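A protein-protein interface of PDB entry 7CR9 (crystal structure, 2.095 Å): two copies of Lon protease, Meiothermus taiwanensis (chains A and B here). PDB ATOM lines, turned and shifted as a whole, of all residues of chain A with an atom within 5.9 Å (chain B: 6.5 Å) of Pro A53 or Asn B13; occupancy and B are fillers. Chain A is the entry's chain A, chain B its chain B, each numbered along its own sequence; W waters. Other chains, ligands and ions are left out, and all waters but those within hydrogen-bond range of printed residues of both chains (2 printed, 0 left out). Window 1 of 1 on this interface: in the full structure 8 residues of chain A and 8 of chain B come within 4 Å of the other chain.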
ATOM      1  N   ARG A  12      16.422 -28.951  -7.280  1.00  0.00           N
ATOM      2  CA  ARG A  12      15.170 -28.222  -7.094  1.00  0.00           C
ATOM      3  C   ARG A  12      14.216 -28.440  -8.262  1.00  0.00           C
ATOM      4  O   ARG A  12      13.044 -28.784  -8.066  1.00  0.00           O
ATOM      5  CB  ARG A  12      15.455 -26.730  -6.920  1.00  0.00           C
ATOM      6  CG  ARG A  12      15.824 -26.306  -5.510  1.00  0.00           C
ATOM      7  CD  ARG A  12      15.895 -24.788  -5.418  1.00  0.00           C
ATOM      8  NE  ARG A  12      16.310 -24.328  -4.096  1.00  0.00           N
ATOM      9  CZ  ARG A  12      15.472 -24.081  -3.095  1.00  0.00           C
ATOM     10  NH1 ARG A  12      14.168 -24.251  -3.262  1.00  0.00           N
ATOM     11  NH2 ARG A  12      15.939 -23.662  -1.928  1.00  0.00           N
ATOM     12  N   ASN A  13      14.700 -28.244  -9.487  1.00  0.00           N
ATOM     13  CA  ASN A  13      13.837 -28.185 -10.663  1.00  0.00           C
ATOM     14  C   ASN A  13      14.525 -28.820 -11.864  1.00  0.00           C
ATOM     15  O   ASN A  13      14.370 -28.367 -13.003  1.00  0.00           O
ATOM     16  CB  ASN A  13      13.437 -26.741 -10.968  1.00  0.00           C
ATOM     17  CG  ASN A  13      12.255 -26.646 -11.914  1.00  0.00           C
ATOM     18  OD1 ASN A  13      11.239 -27.313 -11.725  1.00  0.00           O
ATOM     19  ND2 ASN A  13      12.386 -25.812 -12.940  1.00  0.00           N
ATOM     20  N   GLN A  50      13.733 -33.031  -6.484  1.00  0.00           N
ATOM     21  CA  GLN A  50      12.712 -32.708  -5.501  1.00  0.00           C
ATOM     22  C   GLN A  50      11.326 -32.794  -6.127  1.00  0.00           C
ATOM     23  O   GLN A  50      11.144 -32.554  -7.324  1.00  0.00           O
ATOM     24  CB  GLN A  50      12.928 -31.304  -4.933  1.00  0.00           C
ATOM     25  CG  GLN A  50      14.179 -31.150  -4.087  1.00  0.00           C
ATOM     26  CD  GLN A  50      14.344 -29.741  -3.553  1.00  0.00           C
ATOM     27  OE1 GLN A  50      15.441 -29.332  -3.177  1.00  0.00           O
ATOM     28  NE2 GLN A  50      13.248 -28.990  -3.516  1.00  0.00           N
ATOM     29  N   ARG A  51      10.340 -33.151  -5.302  1.00  0.00           N
ATOM     30  CA  ARG A  51       8.958 -33.125  -5.766  1.00  0.00           C
ATOM     31  C   ARG A  51       8.433 -31.699  -5.867  1.00  0.00           C
ATOM     32  O   ARG A  51       7.575 -31.413  -6.711  1.00  0.00           O
ATOM     33  CB  ARG A  51       8.073 -33.956  -4.836  1.00  0.00           C
ATOM     34  CG  ARG A  51       8.392 -35.442  -4.843  1.00  0.00           C
ATOM     35  CD  ARG A  51       7.593 -36.185  -3.782  1.00  0.00           C
ATOM     36  NE  ARG A  51       8.034 -37.570  -3.636  1.00  0.00           N
ATOM     37  CZ  ARG A  51       7.615 -38.571  -4.403  1.00  0.00           C
ATOM     38  NH1 ARG A  51       6.736 -38.348  -5.371  1.00  0.00           N
ATOM     39  NH2 ARG A  51       8.071 -39.800  -4.199  1.00  0.00           N
ATOM     40  N   ASP A  52       8.942 -30.797  -5.030  1.00  0.00           N
ATOM     41  CA  ASP A  52       8.488 -29.410  -4.975  1.00  0.00           C
ATOM     42  C   ASP A  52       9.716 -28.515  -5.037  1.00  0.00           C
ATOM     43  O   ASP A  52      10.556 -28.553  -4.115  1.00  0.00           O
ATOM     44  CB  ASP A  52       7.678 -29.157  -3.698  1.00  0.00           C
ATOM     45  CG  ASP A  52       7.068 -27.766  -3.649  1.00  0.00           C
ATOM     46  OD1 ASP A  52       7.294 -26.964  -4.580  1.00  0.00           O
ATOM     47  OD2 ASP A  52       6.353 -27.474  -2.667  1.00  0.00           O
ATOM     48  N   PRO A  53       9.879 -27.710  -6.091  1.00  0.00           N
ATOM     49  CA  PRO A  53      11.082 -26.865  -6.194  1.00  0.00           C
ATOM     50  C   PRO A  53      11.226 -25.852  -5.070  1.00  0.00           C
ATOM     51  O   PRO A  53      12.350 -25.412  -4.796  1.00  0.00           O
ATOM     52  CB  PRO A  53      10.908 -26.165  -7.551  1.00  0.00           C
ATOM     53  CG  PRO A  53       9.934 -27.011  -8.307  1.00  0.00           C
ATOM     54  CD  PRO A  53       9.018 -27.603  -7.281  1.00  0.00           C
ATOM     55  N   GLU A  54      10.134 -25.463  -4.414  1.00  0.00           N
ATOM     56  CA  GLU A  54      10.191 -24.423  -3.395  1.00  0.00           C
ATOM     57  C   GLU A  54      10.675 -24.931  -2.041  1.00  0.00           C
ATOM     58  O   GLU A  54      10.945 -24.111  -1.156  1.00  0.00           O
ATOM     59  CB  GLU A  54       8.820 -23.757  -3.257  1.00  0.00           C
ATOM     60  CG  GLU A  54       8.524 -22.783  -4.391  1.00  0.00           C
ATOM     61  CD  GLU A  54       7.103 -22.256  -4.372  1.00  0.00           C
ATOM     62  OE1 GLU A  54       6.265 -22.823  -3.640  1.00  0.00           O
ATOM     63  OE2 GLU A  54       6.823 -21.276  -5.096  1.00  0.00           O
ATOM     64  N   VAL A  55      10.785 -26.245  -1.852  1.00  0.00           N
ATOM     65  CA  VAL A  55      11.249 -26.786  -0.578  1.00  0.00           C
ATOM     66  C   VAL A  55      12.733 -26.474  -0.426  1.00  0.00           C
ATOM     67  O   VAL A  55      13.550 -26.836  -1.280  1.00  0.00           O
ATOM     68  CB  VAL A  55      10.983 -28.295  -0.493  1.00  0.00           C
ATOM     69  CG1 VAL A  55      11.686 -28.891   0.717  1.00  0.00           C
ATOM     70  CG2 VAL A  55       9.486 -28.567  -0.433  1.00  0.00           C
ATOM     71  N   ASP A  56      13.090 -25.798   0.671  1.00  0.00           N
ATOM     72  CA  ASP A  56      14.458 -25.311   0.828  1.00  0.00           C
ATOM     73  C   ASP A  56      15.401 -26.388   1.354  1.00  0.00           C
ATOM     74  O   ASP A  56      16.546 -26.482   0.901  1.00  0.00           O
ATOM     75  CB  ASP A  56      14.475 -24.097   1.758  1.00  0.00           C
ATOM     76  CG  ASP A  56      13.977 -22.834   1.080  1.00  0.00           C
ATOM     77  OD1 ASP A  56      14.168 -22.702  -0.147  1.00  0.00           O
ATOM     78  OD2 ASP A  56      13.395 -21.973   1.773  1.00  0.00           O
ATOM     79  N   VAL A 174       9.541 -31.579 -14.412  1.00  0.00           N
ATOM     80  CA  VAL A 174      10.239 -32.552 -13.574  1.00  0.00           C
ATOM     81  C   VAL A 174       9.443 -33.850 -13.499  1.00  0.00           C
ATOM     82  O   VAL A 174       9.994 -34.947 -13.645  1.00  0.00           O
ATOM     83  CB  VAL A 174      10.502 -31.963 -12.176  1.00  0.00           C
ATOM     84  CG1 VAL A 174      10.865 -33.066 -11.192  1.00  0.00           C
ATOM     85  CG2 VAL A 174      11.607 -30.920 -12.241  1.00  0.00           C
ATOM     86  N   LEU B  11       8.880 -15.106  -6.255  1.00  0.00           N
ATOM     87  CA  LEU B  11       8.314 -16.435  -6.055  1.00  0.00           C
ATOM     88  C   LEU B  11       9.042 -17.424  -6.954  1.00  0.00           C
ATOM     89  O   LEU B  11       9.093 -17.236  -8.175  1.00  0.00           O
ATOM     90  CB  LEU B  11       6.813 -16.438  -6.339  1.00  0.00           C
ATOM     91  CG  LEU B  11       6.029 -15.357  -5.593  1.00  0.00           C
ATOM     92  CD1 LEU B  11       4.676 -15.136  -6.244  1.00  0.00           C
ATOM     93  CD2 LEU B  11       5.874 -15.720  -4.123  1.00  0.00           C
ATOM     94  N   ARG B  12       9.598 -18.476  -6.348  1.00  0.00           N
ATOM     95  CA  ARG B  12      10.419 -19.425  -7.094  1.00  0.00           C
ATOM     96  C   ARG B  12       9.607 -20.149  -8.162  1.00  0.00           C
ATOM     97  O   ARG B  12      10.013 -20.215  -9.329  1.00  0.00           O
ATOM     98  CB  ARG B  12      11.051 -20.435  -6.135  1.00  0.00           C
ATOM     99  CG  ARG B  12      12.296 -19.943  -5.417  1.00  0.00           C
ATOM    100  CD  ARG B  12      12.962 -21.083  -4.661  1.00  0.00           C
ATOM    101  NE  ARG B  12      14.114 -20.638  -3.883  1.00  0.00           N
ATOM    102  CZ  ARG B  12      15.357 -20.581  -4.350  1.00  0.00           C
ATOM    103  NH1 ARG B  12      15.617 -20.941  -5.599  1.00  0.00           N
ATOM    104  NH2 ARG B  12      16.341 -20.162  -3.566  1.00  0.00           N
ATOM    105  N   ASN B  13       8.458 -20.702  -7.781  1.00  0.00           N
ATOM    106  CA  ASN B  13       7.708 -21.611  -8.642  1.00  0.00           C
ATOM    107  C   ASN B  13       6.212 -21.402  -8.467  1.00  0.00           C
ATOM    108  O   ASN B  13       5.423 -22.352  -8.499  1.00  0.00           O
ATOM    109  CB  ASN B  13       8.088 -23.065  -8.359  1.00  0.00           C
ATOM    110  CG  ASN B  13       7.612 -24.017  -9.440  1.00  0.00           C
ATOM    111  OD1 ASN B  13       7.817 -23.778 -10.629  1.00  0.00           O
ATOM    112  ND2 ASN B  13       6.965 -25.102  -9.028  1.00  0.00           N
ATOM    113  N   THR B  14       5.796 -20.153  -8.278  1.00  0.00           N
ATOM    114  CA  THR B  14       4.393 -19.846  -8.050  1.00  0.00           C
ATOM    115  C   THR B  14       4.022 -18.565  -8.778  1.00  0.00           C
ATOM    116  O   THR B  14       4.797 -17.604  -8.797  1.00  0.00           O
ATOM    117  CB  THR B  14       4.089 -19.698  -6.551  1.00  0.00           C
ATOM    118  OG1 THR B  14       4.597 -20.837  -5.844  1.00  0.00           O
ATOM    119  CG2 THR B  14       2.592 -19.595  -6.314  1.00  0.00           C
ATOM    120  N   VAL B  15       2.836 -18.560  -9.379  1.00  0.00           N
ATOM    121  CA  VAL B  15       2.231 -17.358  -9.938  1.00  0.00           C
ATOM    122  C   VAL B  15       0.984 -17.063  -9.119  1.00  0.00           C
ATOM    123  O   VAL B  15       0.077 -17.900  -9.031  1.00  0.00           O
ATOM    124  CB  VAL B  15       1.887 -17.525 -11.424  1.00  0.00           C
ATOM    125  CG1 VAL B  15       1.089 -16.326 -11.922  1.00  0.00           C
ATOM    126  CG2 VAL B  15       3.152 -17.702 -12.246  1.00  0.00           C
ATOM    127  N   ALA B  49       6.719 -13.655  -9.970  1.00  0.00           N
ATOM    128  CA  ALA B  49       7.262 -14.988 -10.182  1.00  0.00           C
ATOM    129  C   ALA B  49       8.642 -14.915 -10.825  1.00  0.00           C
ATOM    130  O   ALA B  49       8.906 -14.057 -11.672  1.00  0.00           O
ATOM    131  CB  ALA B  49       6.323 -15.812 -11.062  1.00  0.00           C
ATOM    132  N   GLN B  50       9.521 -15.825 -10.418  1.00  0.00           N
ATOM    133  CA  GLN B  50      10.812 -15.972 -11.070  1.00  0.00           C
ATOM    134  C   GLN B  50      10.657 -16.705 -12.397  1.00  0.00           C
ATOM    135  O   GLN B  50       9.769 -17.545 -12.567  1.00  0.00           O
ATOM    136  CB  GLN B  50      11.790 -16.735 -10.173  1.00  0.00           C
ATOM    137  CG  GLN B  50      12.181 -16.002  -8.900  1.00  0.00           C
ATOM    138  CD  GLN B  50      13.173 -16.783  -8.059  1.00  0.00           C
ATOM    139  OE1 GLN B  50      13.320 -16.535  -6.862  1.00  0.00           O
ATOM    140  NE2 GLN B  50      13.863 -17.732  -8.683  1.00  0.00           N
ATOM    141  N   PRO B  53      13.064 -21.256 -11.315  1.00  0.00           N
ATOM    142  CA  PRO B  53      12.928 -21.534  -9.874  1.00  0.00           C
ATOM    143  C   PRO B  53      14.250 -21.748  -9.158  1.00  0.00           C
ATOM    144  O   PRO B  53      14.313 -21.558  -7.937  1.00  0.00           O
ATOM    145  CB  PRO B  53      12.066 -22.806  -9.839  1.00  0.00           C
ATOM    146  CG  PRO B  53      11.396 -22.866 -11.175  1.00  0.00           C
ATOM    147  CD  PRO B  53      12.346 -22.239 -12.144  1.00  0.00           C
ATOM    148  N   GLU B  54      15.306 -22.138  -9.869  1.00  0.00           N
ATOM    149  CA  GLU B  54      16.574 -22.461  -9.229  1.00  0.00           C
ATOM    150  C   GLU B  54      17.413 -21.234  -8.889  1.00  0.00           C
ATOM    151  O   GLU B  54      18.403 -21.369  -8.161  1.00  0.00           O
ATOM    152  CB  GLU B  54      17.373 -23.412 -10.125  1.00  0.00           C
ATOM    153  CG  GLU B  54      16.601 -24.673 -10.490  1.00  0.00           C
ATOM    154  CD  GLU B  54      17.489 -25.774 -11.034  1.00  0.00           C
ATOM    155  OE1 GLU B  54      17.433 -26.902 -10.498  1.00  0.00           O
ATOM    156  OE2 GLU B  54      18.236 -25.517 -12.002  1.00  0.00           O
ATOM    157  N   THR B 173       2.010 -24.700 -15.565  1.00  0.00           N
ATOM    158  CA  THR B 173       3.343 -24.214 -15.247  1.00  0.00           C
ATOM    159  C   THR B 173       3.304 -22.724 -14.918  1.00  0.00           C
ATOM    160  O   THR B 173       2.309 -22.028 -15.146  1.00  0.00           O
ATOM    161  CB  THR B 173       4.303 -24.471 -16.407  1.00  0.00           C
ATOM    162  OG1 THR B 173       3.833 -23.793 -17.579  1.00  0.00           O
ATOM    163  CG2 THR B 173       4.410 -25.962 -16.694  1.00  0.00           C
ATOM    164  N   VAL B 174       4.414 -22.238 -14.357  1.00  0.00           N
ATOM    165  CA  VAL B 174       4.559 -20.809 -14.097  1.00  0.00           C
ATOM    166  C   VAL B 174       4.396 -20.016 -15.387  1.00  0.00           C
ATOM    167  O   VAL B 174       3.670 -19.015 -15.434  1.00  0.00           O
ATOM    168  CB  VAL B 174       5.913 -20.523 -13.424  1.00  0.00           C
ATOM    169  CG1 VAL B 174       6.254 -19.042 -13.511  1.00  0.00           C
ATOM    170  CG2 VAL B 174       5.889 -20.985 -11.976  1.00  0.00           C
HETATM  171  O   HOH W   1      13.958 -20.098  -1.194  1.00  0.00           O
HETATM  172  O   HOH W   2       5.666 -25.193  -6.178  1.00  0.00           O
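OE1 of Glu B54 sits at hydrogen-bond distance from N of Asn A13 (3.2 Å).
OE1 of Glu A54 sits close to OG1 of Thr B14, at 3.4 Å.
The side-chain carboxylate (OE2) of Glu A54 is in hydrogen-bond range of the backbone NH (N) of Asn B13 (3.2 Å).
NH2 of Arg A12 lies within salt-bridge range of OD1 of Asp A56, 2.7 Å away.
The side-chain carboxylate of Asp A52 lies close to the backbone NH of Glu A54, at 3.2 Å.
The guanidinium group of Arg A12 is in hydrogen-bond range of the backbone carbonyl oxygen of Val A55.
O of Pro A53 sits at hydrogen-bond distance from NH1 of Arg A12, at 2.6 Å.
O of Pro B53 sits at hydrogen-bond distance from NH1 of Arg B12 (2.7 Å).
Among the printed residues, merely in contact across the chains: Asn A13 with Pro B53 (3.6 Å), Pro A53 with Asn B13 (3.6 Å), Arg A12 with Arg B12 (3.7 Å), Glu A54 with Arg B12 (3.9 Å) and Arg A12 with Glu B54 (3.9 Å).
Asp A52 touches none of the printed residues of chain B.
Of chain B, only Asn B13 comes within 4 Å of Pro A53.
Printed residues of chain A within 4 Å of Arg B12: Arg A12 and Glu A54.
Printed residues of chain A within 4 Å of Thr B14: Glu A54.
The nearest residue of chain A that does not touch Asn B13 is Asp A52 (4.8 Å).
The nearest printed residue of chain B that does not touch Asn A13 is Asn B13 (5.0 Å).
Of the 10 printed residues of chain A, 4 touch a printed residue of chain B.
Hydrophobic or aromatic side chains of chain A within 4 Å of the printed part of chain B: Pro A53.
Of the 11 printed residues of chain B, 5 touch a printed residue of chain A.
Printed residues of chain B that touch a printed residue of chain A: Arg B12, Asn B13, Thr B14, Pro B53 and Glu B54.
Hydrophobic or aromatic side chains of chain B within 4 Å of the printed part of chain A: Pro B53.
Among the printed residues, 8 pairs touch across the chains.
Arg B12 touches its own counterpart, Arg A12.
Arg A12 touches Glu B54, and with the chains exchanged Glu A54 touches Arg B12.
Asn A13 touches Pro B53, and with the chains exchanged Pro A53 touches Asn B13.
Asn A13 touches Glu B54, and with the chains exchanged Glu A54 touches Asn B13.
Of the 8 pairs that touch across the chains among the printed residues, 7 have their exchanged pair printed and touching as well.
Water W1 lies within hydrogen-bond range of NE of Arg B12 (2.7 Å) and OD1 of Asp A56 (2.8 Å).
Water W2 lies within hydrogen-bond range of the side-chain carboxylate of Asp A52 and the side-chain amide nitrogen of Asn B13.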
